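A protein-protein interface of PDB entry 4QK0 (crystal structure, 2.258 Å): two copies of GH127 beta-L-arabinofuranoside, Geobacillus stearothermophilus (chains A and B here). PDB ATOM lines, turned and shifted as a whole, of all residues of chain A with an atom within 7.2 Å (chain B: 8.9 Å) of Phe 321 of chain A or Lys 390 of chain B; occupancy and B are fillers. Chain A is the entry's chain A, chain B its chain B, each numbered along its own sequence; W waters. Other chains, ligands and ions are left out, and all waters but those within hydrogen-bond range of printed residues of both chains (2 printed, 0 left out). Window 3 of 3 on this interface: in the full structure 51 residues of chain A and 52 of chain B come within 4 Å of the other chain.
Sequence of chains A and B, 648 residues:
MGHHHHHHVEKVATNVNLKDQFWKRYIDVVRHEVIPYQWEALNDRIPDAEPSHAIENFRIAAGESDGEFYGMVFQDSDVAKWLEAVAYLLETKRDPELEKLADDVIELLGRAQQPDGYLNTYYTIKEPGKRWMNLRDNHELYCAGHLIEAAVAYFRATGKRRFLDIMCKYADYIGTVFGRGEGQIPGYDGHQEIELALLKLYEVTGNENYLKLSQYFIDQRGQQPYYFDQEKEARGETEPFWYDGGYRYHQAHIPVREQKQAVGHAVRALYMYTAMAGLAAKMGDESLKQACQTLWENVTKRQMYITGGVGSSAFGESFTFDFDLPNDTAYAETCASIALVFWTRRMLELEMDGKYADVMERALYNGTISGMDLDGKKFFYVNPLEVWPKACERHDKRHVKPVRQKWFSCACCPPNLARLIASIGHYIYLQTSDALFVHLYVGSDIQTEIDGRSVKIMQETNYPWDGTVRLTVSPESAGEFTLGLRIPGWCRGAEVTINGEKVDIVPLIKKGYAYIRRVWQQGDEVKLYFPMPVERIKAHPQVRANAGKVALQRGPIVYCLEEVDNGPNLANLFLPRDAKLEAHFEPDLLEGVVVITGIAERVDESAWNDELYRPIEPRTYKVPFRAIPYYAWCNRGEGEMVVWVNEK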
ATOM      1  N   ARG A 248     -10.285  23.302  24.077  1.00  0.00           N
ATOM      2  CA  ARG A 248     -11.291  24.151  23.419  1.00  0.00           C
ATOM      3  C   ARG A 248     -12.635  23.472  23.303  1.00  0.00           C
ATOM      4  O   ARG A 248     -13.673  24.128  23.356  1.00  0.00           O
ATOM      5  CB  ARG A 248     -10.837  24.535  22.017  1.00  0.00           C
ATOM      6  CG  ARG A 248      -9.614  25.436  22.041  1.00  0.00           C
ATOM      7  CD  ARG A 248      -8.893  25.394  20.707  1.00  0.00           C
ATOM      8  NE  ARG A 248      -9.716  25.961  19.654  1.00  0.00           N
ATOM      9  CZ  ARG A 248      -9.694  27.241  19.279  1.00  0.00           C
ATOM     10  NH1 ARG A 248      -8.916  28.109  19.924  1.00  0.00           N
ATOM     11  NH2 ARG A 248     -10.469  27.662  18.253  1.00  0.00           N
ATOM     12  N   GLN A 261     -13.680  34.520  21.271  1.00  0.00           N
ATOM     13  CA  GLN A 261     -14.429  33.782  20.246  1.00  0.00           C
ATOM     14  C   GLN A 261     -15.090  32.580  20.824  1.00  0.00           C
ATOM     15  O   GLN A 261     -14.539  31.900  21.689  1.00  0.00           O
ATOM     16  CB  GLN A 261     -13.530  33.257  19.108  1.00  0.00           C
ATOM     17  CG  GLN A 261     -12.983  34.332  18.193  1.00  0.00           C
ATOM     18  CD  GLN A 261     -11.768  34.979  18.806  1.00  0.00           C
ATOM     19  OE1 GLN A 261     -10.989  34.313  19.472  1.00  0.00           O
ATOM     20  NE2 GLN A 261     -11.594  36.267  18.576  1.00  0.00           N
ATOM     21  N   ALA A 262     -16.249  32.281  20.278  1.00  0.00           N
ATOM     22  CA  ALA A 262     -16.905  31.011  20.532  1.00  0.00           C
ATOM     23  C   ALA A 262     -16.124  29.918  19.840  1.00  0.00           C
ATOM     24  O   ALA A 262     -15.773  30.038  18.675  1.00  0.00           O
ATOM     25  CB  ALA A 262     -18.318  31.041  20.011  1.00  0.00           C
ATOM     26  N   VAL A 263     -15.792  28.894  20.608  1.00  0.00           N
ATOM     27  CA  VAL A 263     -15.079  27.713  20.137  1.00  0.00           C
ATOM     28  C   VAL A 263     -15.691  26.481  20.783  1.00  0.00           C
ATOM     29  O   VAL A 263     -16.374  26.572  21.815  1.00  0.00           O
ATOM     30  CB  VAL A 263     -13.585  27.754  20.485  1.00  0.00           C
ATOM     31  CG1 VAL A 263     -12.927  28.996  19.891  1.00  0.00           C
ATOM     32  CG2 VAL A 263     -13.361  27.745  21.980  1.00  0.00           C
ATOM     33  N   ASN A 298     -19.728  37.816  18.857  1.00  0.00           N
ATOM     34  CA  ASN A 298     -19.046  36.868  18.037  1.00  0.00           C
ATOM     35  C   ASN A 298     -20.018  35.758  17.563  1.00  0.00           C
ATOM     36  O   ASN A 298     -20.039  35.396  16.382  1.00  0.00           O
ATOM     37  CB  ASN A 298     -17.901  36.245  18.754  1.00  0.00           C
ATOM     38  CG  ASN A 298     -17.092  35.319  17.830  1.00  0.00           C
ATOM     39  OD1 ASN A 298     -17.009  34.105  18.031  1.00  0.00           O
ATOM     40  ND2 ASN A 298     -16.428  35.924  16.845  1.00  0.00           N
ATOM     41  N   ARG A 302     -21.189  36.443  13.776  1.00  0.00           N
ATOM     42  CA  ARG A 302     -20.194  35.745  12.965  1.00  0.00           C
ATOM     43  C   ARG A 302     -20.360  34.275  12.896  1.00  0.00           C
ATOM     44  O   ARG A 302     -19.835  33.714  11.976  1.00  0.00           O
ATOM     45  CB  ARG A 302     -18.790  36.097  13.430  1.00  0.00           C
ATOM     46  CG  ARG A 302     -18.589  37.581  13.378  1.00  0.00           C
ATOM     47  CD  ARG A 302     -17.170  37.960  13.480  1.00  0.00           C
ATOM     48  NE  ARG A 302     -16.974  39.363  13.147  1.00  0.00           N
ATOM     49  CZ  ARG A 302     -15.774  39.896  12.933  1.00  0.00           C
ATOM     50  NH1 ARG A 302     -14.685  39.131  12.984  1.00  0.00           N
ATOM     51  NH2 ARG A 302     -15.662  41.182  12.636  1.00  0.00           N
ATOM     52  N   GLN A 303     -21.038  33.639  13.853  1.00  0.00           N
ATOM     53  CA  GLN A 303     -21.097  32.163  13.878  1.00  0.00           C
ATOM     54  C   GLN A 303     -22.486  31.605  14.108  1.00  0.00           C
ATOM     55  O   GLN A 303     -22.649  30.585  14.740  1.00  0.00           O
ATOM     56  CB  GLN A 303     -20.133  31.577  14.868  1.00  0.00           C
ATOM     57  CG  GLN A 303     -18.679  31.949  14.576  1.00  0.00           C
ATOM     58  CD  GLN A 303     -17.732  31.086  15.390  1.00  0.00           C
ATOM     59  OE1 GLN A 303     -17.583  29.891  15.146  1.00  0.00           O
ATOM     60  NE2 GLN A 303     -17.155  31.672  16.449  1.00  0.00           N
ATOM     61  N   SER A 312     -21.139  24.537  13.276  1.00  0.00           N
ATOM     62  CA  SER A 312     -20.911  24.409  11.840  1.00  0.00           C
ATOM     63  C   SER A 312     -20.102  23.161  11.476  1.00  0.00           C
ATOM     64  O   SER A 312     -19.821  22.966  10.332  1.00  0.00           O
ATOM     65  CB  SER A 312     -20.165  25.659  11.339  1.00  0.00           C
ATOM     66  OG  SER A 312     -18.921  25.757  12.022  1.00  0.00           O
ATOM     67  N   SER A 318     -19.505  21.415  16.883  1.00  0.00           N
ATOM     68  CA  SER A 318     -18.811  22.562  17.362  1.00  0.00           C
ATOM     69  C   SER A 318     -18.861  23.779  16.459  1.00  0.00           C
ATOM     70  O   SER A 318     -19.179  23.721  15.246  1.00  0.00           O
ATOM     71  CB  SER A 318     -17.352  22.150  17.603  1.00  0.00           C
ATOM     72  OG  SER A 318     -16.808  21.632  16.413  1.00  0.00           O
ATOM     73  N   PHE A 319     -18.549  24.906  17.095  1.00  0.00           N
ATOM     74  CA  PHE A 319     -18.136  26.076  16.396  1.00  0.00           C
ATOM     75  C   PHE A 319     -16.861  25.786  15.629  1.00  0.00           C
ATOM     76  O   PHE A 319     -15.999  24.992  16.043  1.00  0.00           O
ATOM     77  CB  PHE A 319     -17.865  27.194  17.373  1.00  0.00           C
ATOM     78  CG  PHE A 319     -19.114  27.746  18.040  1.00  0.00           C
ATOM     79  CD1 PHE A 319     -19.988  28.533  17.348  1.00  0.00           C
ATOM     80  CD2 PHE A 319     -19.410  27.430  19.356  1.00  0.00           C
ATOM     81  CE1 PHE A 319     -21.130  29.046  17.952  1.00  0.00           C
ATOM     82  CE2 PHE A 319     -20.571  27.929  19.970  1.00  0.00           C
ATOM     83  CZ  PHE A 319     -21.436  28.730  19.276  1.00  0.00           C
ATOM     84  N   THR A 320     -16.729  26.461  14.498  1.00  0.00           N
ATOM     85  CA  THR A 320     -15.453  26.538  13.804  1.00  0.00           C
ATOM     86  C   THR A 320     -14.889  27.943  13.988  1.00  0.00           C
ATOM     87  O   THR A 320     -14.051  28.162  14.862  1.00  0.00           O
ATOM     88  CB  THR A 320     -15.581  26.157  12.323  1.00  0.00           C
ATOM     89  OG1 THR A 320     -16.607  26.930  11.676  1.00  0.00           O
ATOM     90  CG2 THR A 320     -15.945  24.696  12.254  1.00  0.00           C
ATOM     91  N   PHE A 321     -15.218  28.863  13.085  1.00  0.00           N
ATOM     92  CA  PHE A 321     -14.626  30.195  13.148  1.00  0.00           C
ATOM     93  C   PHE A 321     -15.500  31.163  12.410  1.00  0.00           C
ATOM     94  O   PHE A 321     -16.442  30.780  11.666  1.00  0.00           O
ATOM     95  CB  PHE A 321     -13.150  30.172  12.620  1.00  0.00           C
ATOM     96  CG  PHE A 321     -13.028  29.701  11.197  1.00  0.00           C
ATOM     97  CD1 PHE A 321     -13.161  30.612  10.135  1.00  0.00           C
ATOM     98  CD2 PHE A 321     -12.888  28.357  10.904  1.00  0.00           C
ATOM     99  CE1 PHE A 321     -13.129  30.187   8.807  1.00  0.00           C
ATOM    100  CE2 PHE A 321     -12.836  27.921   9.567  1.00  0.00           C
ATOM    101  CZ  PHE A 321     -12.955  28.858   8.532  1.00  0.00           C
ATOM    102  N   ASP A 322     -15.150  32.432  12.512  1.00  0.00           N
ATOM    103  CA  ASP A 322     -15.971  33.479  11.906  1.00  0.00           C
ATOM    104  C   ASP A 322     -16.342  33.258  10.447  1.00  0.00           C
ATOM    105  O   ASP A 322     -15.494  33.015   9.598  1.00  0.00           O
ATOM    106  CB  ASP A 322     -15.251  34.808  12.019  1.00  0.00           C
ATOM    107  CG  ASP A 322     -15.069  35.258  13.496  1.00  0.00           C
ATOM    108  OD1 ASP A 322     -15.475  34.524  14.444  1.00  0.00           O
ATOM    109  OD2 ASP A 322     -14.482  36.339  13.685  1.00  0.00           O
ATOM    110  N   PHE A 323     -17.631  33.395  10.183  1.00  0.00           N
ATOM    111  CA  PHE A 323     -18.190  33.409   8.869  1.00  0.00           C
ATOM    112  C   PHE A 323     -18.187  32.030   8.135  1.00  0.00           C
ATOM    113  O   PHE A 323     -18.560  31.994   6.972  1.00  0.00           O
ATOM    114  CB  PHE A 323     -17.518  34.458   7.999  1.00  0.00           C
ATOM    115  CG  PHE A 323     -17.553  35.855   8.553  1.00  0.00           C
ATOM    116  CD1 PHE A 323     -18.753  36.534   8.719  1.00  0.00           C
ATOM    117  CD2 PHE A 323     -16.365  36.527   8.819  1.00  0.00           C
ATOM    118  CE1 PHE A 323     -18.764  37.853   9.142  1.00  0.00           C
ATOM    119  CE2 PHE A 323     -16.370  37.860   9.252  1.00  0.00           C
ATOM    120  CZ  PHE A 323     -17.578  38.508   9.435  1.00  0.00           C
ATOM    121  N   ASP A 324     -17.770  30.949   8.805  1.00  0.00           N
ATOM    122  CA  ASP A 324     -17.787  29.580   8.264  1.00  0.00           C
ATOM    123  C   ASP A 324     -19.116  28.920   8.572  1.00  0.00           C
ATOM    124  O   ASP A 324     -19.316  28.307   9.613  1.00  0.00           O
ATOM    125  CB  ASP A 324     -16.618  28.749   8.827  1.00  0.00           C
ATOM    126  CG  ASP A 324     -16.605  27.293   8.302  1.00  0.00           C
ATOM    127  OD1 ASP A 324     -16.896  27.089   7.132  1.00  0.00           O
ATOM    128  OD2 ASP A 324     -16.304  26.358   9.058  1.00  0.00           O
ATOM    129  N   LEU A 325     -20.040  29.095   7.666  1.00  0.00           N
ATOM    130  CA  LEU A 325     -21.429  28.687   7.892  1.00  0.00           C
ATOM    131  C   LEU A 325     -22.011  27.919   6.711  1.00  0.00           C
ATOM    132  O   LEU A 325     -22.946  28.380   6.038  1.00  0.00           O
ATOM    133  CB  LEU A 325     -22.254  29.950   8.118  1.00  0.00           C
ATOM    134  CG  LEU A 325     -21.902  30.646   9.432  1.00  0.00           C
ATOM    135  CD1 LEU A 325     -22.488  32.033   9.430  1.00  0.00           C
ATOM    136  CD2 LEU A 325     -22.392  29.868  10.652  1.00  0.00           C
ATOM    137  N   ARG A 544     -18.890  32.880   2.916  1.00  0.00           N
ATOM    138  CA  ARG A 544     -18.558  32.320   1.649  1.00  0.00           C
ATOM    139  C   ARG A 544     -19.622  31.373   1.118  1.00  0.00           C
ATOM    140  O   ARG A 544     -19.912  31.426  -0.049  1.00  0.00           O
ATOM    141  CB  ARG A 544     -17.168  31.671   1.743  1.00  0.00           C
ATOM    142  CG  ARG A 544     -16.245  32.884   1.894  1.00  0.00           C
ATOM    143  CD  ARG A 544     -14.781  32.850   2.249  1.00  0.00           C
ATOM    144  NE  ARG A 544     -14.469  34.211   2.671  1.00  0.00           N
ATOM    145  CZ  ARG A 544     -13.267  34.728   2.855  1.00  0.00           C
ATOM    146  NH1 ARG A 544     -12.175  34.082   2.565  1.00  0.00           N
ATOM    147  NH2 ARG A 544     -13.177  35.971   3.263  1.00  0.00           N
ATOM    148  N   VAL B 387      -9.896  26.586  -2.504  1.00  0.00           N
ATOM    149  CA  VAL B 387      -9.197  26.638  -1.236  1.00  0.00           C
ATOM    150  C   VAL B 387      -9.495  27.962  -0.542  1.00  0.00           C
ATOM    151  O   VAL B 387      -9.371  29.042  -1.137  1.00  0.00           O
ATOM    152  CB  VAL B 387      -7.711  26.490  -1.444  1.00  0.00           C
ATOM    153  CG1 VAL B 387      -6.952  26.656  -0.150  1.00  0.00           C
ATOM    154  CG2 VAL B 387      -7.412  25.094  -1.949  1.00  0.00           C
ATOM    155  N   TRP B 388      -9.934  27.854   0.716  1.00  0.00           N
ATOM    156  CA  TRP B 388      -9.956  28.978   1.722  1.00  0.00           C
ATOM    157  C   TRP B 388      -9.083  28.508   2.869  1.00  0.00           C
ATOM    158  O   TRP B 388      -9.477  27.625   3.592  1.00  0.00           O
ATOM    159  CB  TRP B 388     -11.377  29.214   2.175  1.00  0.00           C
ATOM    160  CG  TRP B 388     -11.588  30.269   3.195  1.00  0.00           C
ATOM    161  CD1 TRP B 388     -10.747  31.299   3.509  1.00  0.00           C
ATOM    162  CD2 TRP B 388     -12.774  30.483   3.957  1.00  0.00           C
ATOM    163  NE1 TRP B 388     -11.318  32.100   4.452  1.00  0.00           N
ATOM    164  CE2 TRP B 388     -12.555  31.632   4.753  1.00  0.00           C
ATOM    165  CE3 TRP B 388     -13.998  29.806   4.069  1.00  0.00           C
ATOM    166  CZ2 TRP B 388     -13.512  32.119   5.663  1.00  0.00           C
ATOM    167  CZ3 TRP B 388     -14.927  30.271   4.966  1.00  0.00           C
ATOM    168  CH2 TRP B 388     -14.672  31.423   5.767  1.00  0.00           C
ATOM    169  N   PRO B 389      -7.845  29.006   2.982  1.00  0.00           N
ATOM    170  CA  PRO B 389      -6.885  28.324   3.878  1.00  0.00           C
ATOM    171  C   PRO B 389      -7.300  28.169   5.310  1.00  0.00           C
ATOM    172  O   PRO B 389      -7.035  27.117   5.900  1.00  0.00           O
ATOM    173  CB  PRO B 389      -5.652  29.206   3.795  1.00  0.00           C
ATOM    174  CG  PRO B 389      -5.695  29.700   2.427  1.00  0.00           C
ATOM    175  CD  PRO B 389      -7.151  30.000   2.162  1.00  0.00           C
ATOM    176  N   LYS B 390      -7.944  29.187   5.858  1.00  0.00           N
ATOM    177  CA  LYS B 390      -8.456  29.125   7.221  1.00  0.00           C
ATOM    178  C   LYS B 390      -9.386  27.903   7.394  1.00  0.00           C
ATOM    179  O   LYS B 390      -9.331  27.226   8.388  1.00  0.00           O
ATOM    180  CB  LYS B 390      -9.248  30.416   7.514  1.00  0.00           C
ATOM    181  CG  LYS B 390      -9.072  31.015   8.902  1.00  0.00           C
ATOM    182  CD  LYS B 390      -9.708  32.420   8.943  1.00  0.00           C
ATOM    183  CE  LYS B 390      -9.572  33.089  10.358  1.00  0.00           C
ATOM    184  NZ  LYS B 390     -10.836  33.730  10.896  1.00  0.00           N
ATOM    185  N   ALA B 391     -10.265  27.679   6.418  1.00  0.00           N
ATOM    186  CA  ALA B 391     -11.189  26.558   6.451  1.00  0.00           C
ATOM    187  C   ALA B 391     -10.577  25.159   6.408  1.00  0.00           C
ATOM    188  O   ALA B 391     -11.250  24.212   6.735  1.00  0.00           O
ATOM    189  CB  ALA B 391     -12.192  26.700   5.339  1.00  0.00           C
ATOM    190  N   CYS B 392      -9.330  25.037   5.968  1.00  0.00           N
ATOM    191  CA  CYS B 392      -8.602  23.776   5.993  1.00  0.00           C
ATOM    192  C   CYS B 392      -8.354  23.232   7.396  1.00  0.00           C
ATOM    193  O   CYS B 392      -7.939  22.102   7.538  1.00  0.00           O
ATOM    194  CB  CYS B 392      -7.276  23.898   5.243  1.00  0.00           C
ATOM    195  SG  CYS B 392      -7.585  24.356   3.486  1.00  0.00           S
ATOM    196  N   GLU B 393      -8.731  23.978   8.417  1.00  0.00           N
ATOM    197  CA  GLU B 393      -8.738  23.456   9.767  1.00  0.00           C
ATOM    198  C   GLU B 393      -9.999  22.686  10.090  1.00  0.00           C
ATOM    199  O   GLU B 393     -10.051  22.013  11.114  1.00  0.00           O
ATOM    200  CB  GLU B 393      -8.582  24.595  10.772  1.00  0.00           C
ATOM    201  CG  GLU B 393      -7.325  25.423  10.475  1.00  0.00           C
ATOM    202  CD  GLU B 393      -6.033  24.755  11.010  1.00  0.00           C
ATOM    203  OE1 GLU B 393      -5.918  24.542  12.231  1.00  0.00           O
ATOM    204  OE2 GLU B 393      -5.128  24.393  10.227  1.00  0.00           O
ATOM    205  N   ARG B 394     -11.052  22.864   9.319  1.00  0.00           N
ATOM    206  CA  ARG B 394     -12.224  22.015   9.505  1.00  0.00           C
ATOM    207  C   ARG B 394     -11.838  20.543   9.358  1.00  0.00           C
ATOM    208  O   ARG B 394     -11.080  20.164   8.490  1.00  0.00           O
ATOM    209  CB  ARG B 394     -13.330  22.300   8.516  1.00  0.00           C
ATOM    210  CG  ARG B 394     -14.017  23.663   8.622  1.00  0.00           C
ATOM    211  CD  ARG B 394     -15.007  23.862   7.495  1.00  0.00           C
ATOM    212  NE  ARG B 394     -15.959  22.769   7.581  1.00  0.00           N
ATOM    213  CZ  ARG B 394     -17.083  22.780   8.259  1.00  0.00           C
ATOM    214  NH1 ARG B 394     -17.483  23.865   8.885  1.00  0.00           N
ATOM    215  NH2 ARG B 394     -17.855  21.690   8.316  1.00  0.00           N
ATOM    216  N   HIS B 395     -12.411  19.706  10.208  1.00  0.00           N
ATOM    217  CA  HIS B 395     -12.206  18.252  10.102  1.00  0.00           C
ATOM    218  C   HIS B 395     -12.563  17.724   8.692  1.00  0.00           C
ATOM    219  O   HIS B 395     -11.852  16.911   8.139  1.00  0.00           O
ATOM    220  CB  HIS B 395     -13.090  17.595  11.115  1.00  0.00           C
ATOM    221  CG  HIS B 395     -12.840  16.139  11.300  1.00  0.00           C
ATOM    222  ND1 HIS B 395     -11.749  15.650  11.972  1.00  0.00           N
ATOM    223  CD2 HIS B 395     -13.612  15.076  11.011  1.00  0.00           C
ATOM    224  CE1 HIS B 395     -11.829  14.333  12.046  1.00  0.00           C
ATOM    225  NE2 HIS B 395     -12.948  13.959  11.455  1.00  0.00           N
ATOM    226  N   ASP B 396     -13.651  18.211   8.123  1.00  0.00           N
ATOM    227  CA  ASP B 396     -14.036  17.747   6.806  1.00  0.00           C
ATOM    228  C   ASP B 396     -13.150  18.335   5.683  1.00  0.00           C
ATOM    229  O   ASP B 396     -13.418  18.049   4.526  1.00  0.00           O
ATOM    230  CB  ASP B 396     -15.531  17.901   6.536  1.00  0.00           C
ATOM    231  CG  ASP B 396     -16.003  19.377   6.473  1.00  0.00           C
ATOM    232  OD1 ASP B 396     -15.132  20.287   6.452  1.00  0.00           O
ATOM    233  OD2 ASP B 396     -17.241  19.639   6.396  1.00  0.00           O
ATOM    234  N   LYS B 397     -12.122  19.128   6.018  1.00  0.00           N
ATOM    235  CA  LYS B 397     -11.189  19.639   5.024  1.00  0.00           C
ATOM    236  C   LYS B 397      -9.745  19.454   5.378  1.00  0.00           C
ATOM    237  O   LYS B 397      -8.891  19.982   4.714  1.00  0.00           O
ATOM    238  CB  LYS B 397     -11.430  21.107   4.758  1.00  0.00           C
ATOM    239  CG  LYS B 397     -12.763  21.330   4.131  1.00  0.00           C
ATOM    240  CD  LYS B 397     -13.022  22.762   3.750  1.00  0.00           C
ATOM    241  CE  LYS B 397     -14.515  22.939   3.456  1.00  0.00           C
ATOM    242  NZ  LYS B 397     -14.773  24.318   3.006  1.00  0.00           N
ATOM    243  N   ARG B 398      -9.475  18.693   6.408  1.00  0.00           N
ATOM    244  CA  ARG B 398      -8.155  18.569   6.900  1.00  0.00           C
ATOM    245  C   ARG B 398      -7.254  17.828   5.887  1.00  0.00           C
ATOM    246  O   ARG B 398      -6.056  17.926   6.012  1.00  0.00           O
ATOM    247  CB  ARG B 398      -8.147  17.850   8.272  1.00  0.00           C
ATOM    248  CG  ARG B 398      -8.402  16.346   8.202  1.00  0.00           C
ATOM    249  CD  ARG B 398      -8.661  15.769   9.589  1.00  0.00           C
ATOM    250  NE  ARG B 398      -8.911  14.321   9.600  1.00  0.00           N
ATOM    251  CZ  ARG B 398     -10.029  13.689   9.261  1.00  0.00           C
ATOM    252  NH1 ARG B 398     -11.086  14.348   8.829  1.00  0.00           N
ATOM    253  NH2 ARG B 398     -10.084  12.356   9.319  1.00  0.00           N
ATOM    254  N   VAL B 400      -7.183  18.569   2.815  1.00  0.00           N
ATOM    255  CA  VAL B 400      -6.735  19.597   1.918  1.00  0.00           C
ATOM    256  C   VAL B 400      -5.580  20.431   2.532  1.00  0.00           C
ATOM    257  O   VAL B 400      -5.762  21.141   3.491  1.00  0.00           O
ATOM    258  CB  VAL B 400      -7.883  20.505   1.552  1.00  0.00           C
ATOM    259  CG1 VAL B 400      -7.406  21.601   0.653  1.00  0.00           C
ATOM    260  CG2 VAL B 400      -9.009  19.717   0.890  1.00  0.00           C
ATOM    261  N   PRO B 402      -3.005  23.474   2.210  1.00  0.00           N
ATOM    262  CA  PRO B 402      -3.051  24.707   1.423  1.00  0.00           C
ATOM    263  C   PRO B 402      -1.736  25.032   0.718  1.00  0.00           C
ATOM    264  O   PRO B 402      -1.730  25.875  -0.159  1.00  0.00           O
ATOM    265  CB  PRO B 402      -3.386  25.776   2.459  1.00  0.00           C
ATOM    266  CG  PRO B 402      -2.939  25.188   3.762  1.00  0.00           C
ATOM    267  CD  PRO B 402      -3.156  23.721   3.661  1.00  0.00           C
ATOM    268  N   GLU B 563      -5.399  34.305  -4.818  1.00  0.00           N
ATOM    269  CA  GLU B 563      -5.441  35.503  -3.967  1.00  0.00           C
ATOM    270  C   GLU B 563      -4.286  36.456  -4.309  1.00  0.00           C
ATOM    271  O   GLU B 563      -4.452  37.653  -4.357  1.00  0.00           O
ATOM    272  CB  GLU B 563      -5.380  35.057  -2.508  1.00  0.00           C
ATOM    273  CG  GLU B 563      -5.346  36.185  -1.480  1.00  0.00           C
ATOM    274  CD  GLU B 563      -5.477  35.704  -0.031  1.00  0.00           C
ATOM    275  OE1 GLU B 563      -5.828  34.515   0.280  1.00  0.00           O
ATOM    276  OE2 GLU B 563      -5.165  36.530   0.836  1.00  0.00           O
ATOM    277  N   GLU B 638       0.941  30.777   0.041  1.00  0.00           N
ATOM    278  CA  GLU B 638      -0.359  30.390   0.527  1.00  0.00           C
ATOM    279  C   GLU B 638      -1.389  31.437   0.202  1.00  0.00           C
ATOM    280  O   GLU B 638      -1.125  32.628   0.260  1.00  0.00           O
ATOM    281  CB  GLU B 638      -0.271  30.148   2.029  1.00  0.00           C
ATOM    282  CG  GLU B 638      -1.489  29.478   2.608  1.00  0.00           C
ATOM    283  CD  GLU B 638      -1.234  28.864   3.988  1.00  0.00           C
ATOM    284  OE1 GLU B 638      -0.156  28.249   4.229  1.00  0.00           O
ATOM    285  OE2 GLU B 638      -2.152  28.916   4.827  1.00  0.00           O
ATOM    286  N   GLY B 639      -2.577  30.982  -0.183  1.00  0.00           N
ATOM    287  CA  GLY B 639      -3.644  31.887  -0.460  1.00  0.00           C
ATOM    288  C   GLY B 639      -4.870  31.169  -0.999  1.00  0.00           C
ATOM    289  O   GLY B 639      -4.821  29.960  -1.291  1.00  0.00           O
ATOM    290  N   GLU B 640      -5.971  31.893  -1.050  1.00  0.00           N
ATOM    291  CA  GLU B 640      -7.181  31.397  -1.649  1.00  0.00           C
ATOM    292  C   GLU B 640      -6.982  31.087  -3.140  1.00  0.00           C
ATOM    293  O   GLU B 640      -6.097  31.672  -3.816  1.00  0.00           O
ATOM    294  CB  GLU B 640      -8.311  32.434  -1.520  1.00  0.00           C
ATOM    295  CG  GLU B 640      -8.744  32.626  -0.093  1.00  0.00           C
ATOM    296  CD  GLU B 640     -10.027  33.448   0.000  1.00  0.00           C
ATOM    297  OE1 GLU B 640     -10.968  33.261  -0.829  1.00  0.00           O
ATOM    298  OE2 GLU B 640     -10.083  34.282   0.911  1.00  0.00           O
HETATM  299  O   HOH W   1     -13.180  34.061   9.057  1.00  0.00           O
HETATM  300  O   HOH W   2     -16.878  24.706   5.324  1.00  0.00           O
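Water W2 lies within hydrogen-bond range of the side-chain carboxylate (OD1) of Asp 324 of chain A (3.0 Å), the guanidinium group (NE) of Arg 394 of chain B (3.1 Å) and the side-chain amino group (NZ) of Lys 397 of chain B (3.2 Å).
Of chain B, only Trp 388 (3.6 Å), Lys 390 (3.8 Å) and Ala 391 (3.6 Å) come within 4 Å of Phe 321 of chain A. Printed residues of chain A within 4 Å of Lys 390 of chain B: Phe 321. Thr 320 of chain A touches just one residue of chain B: Arg 394. Asp 324 of chain A touches just one residue of chain B: Arg 394 (2.8 Å). Of the printed residues of chain A, Arg 394 of chain B touches Ser 312, Thr 320 and Asp 324. Gly 639 of chain B touches none of the printed residues of chain A.
The backbone carbonyl oxygen of Ser 312 of chain A lies within hydrogen-bond range of the guanidinium group of Arg 394 of chain B (2.9 Å). OD2 of Asp 324 of chain A is in salt-bridge range of NH1 of Arg 394 of chain B (2.8 Å). NH1 of Arg 544 of chain A is in salt-bridge range of OE2 of Glu 640 of chain B, 2.7 Å away. The guanidinium group (NH1) of Arg 544 of chain A sits close to the indole nitrogen (NE1) of Trp 388 of chain B.
No position is printed for both chains. Of the 8 pairs that touch across the chains among the printed residues, none has its exchanged pair printed and touching as well.
The guanidinium group (NE) of Arg 394 of chain B is in salt-bridge range of the side-chain carboxylate (OD1) of Asp 396 of chain B, at 2.8 Å.
Printed residues of chain B that touch a printed residue of chain A: Trp 388, Lys 390, Ala 391, Arg 394 and Glu 640. Along chain B the printed residues that touch a printed residue of chain A span positions 388 to 640. Printed residues of chain A that touch a printed residue of chain B: Ser 312, Thr 320, Phe 321, Asp 324 and Arg 544. Hydrophobic or aromatic side chains of chain A within 4 Å of the printed part of chain B: Phe 321. Along chain A the printed residues that touch a printed residue of chain B span positions 312 to 544. Among the printed residues, Asp or Glu carboxylates within 4 Å of a Lys or Arg side-chain nitrogen of the other chain: Asp 324 of chain A with Arg 394 of chain B (2.8 Å) and Arg 544 of chain A with Glu 640 of chain B (2.7 Å).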
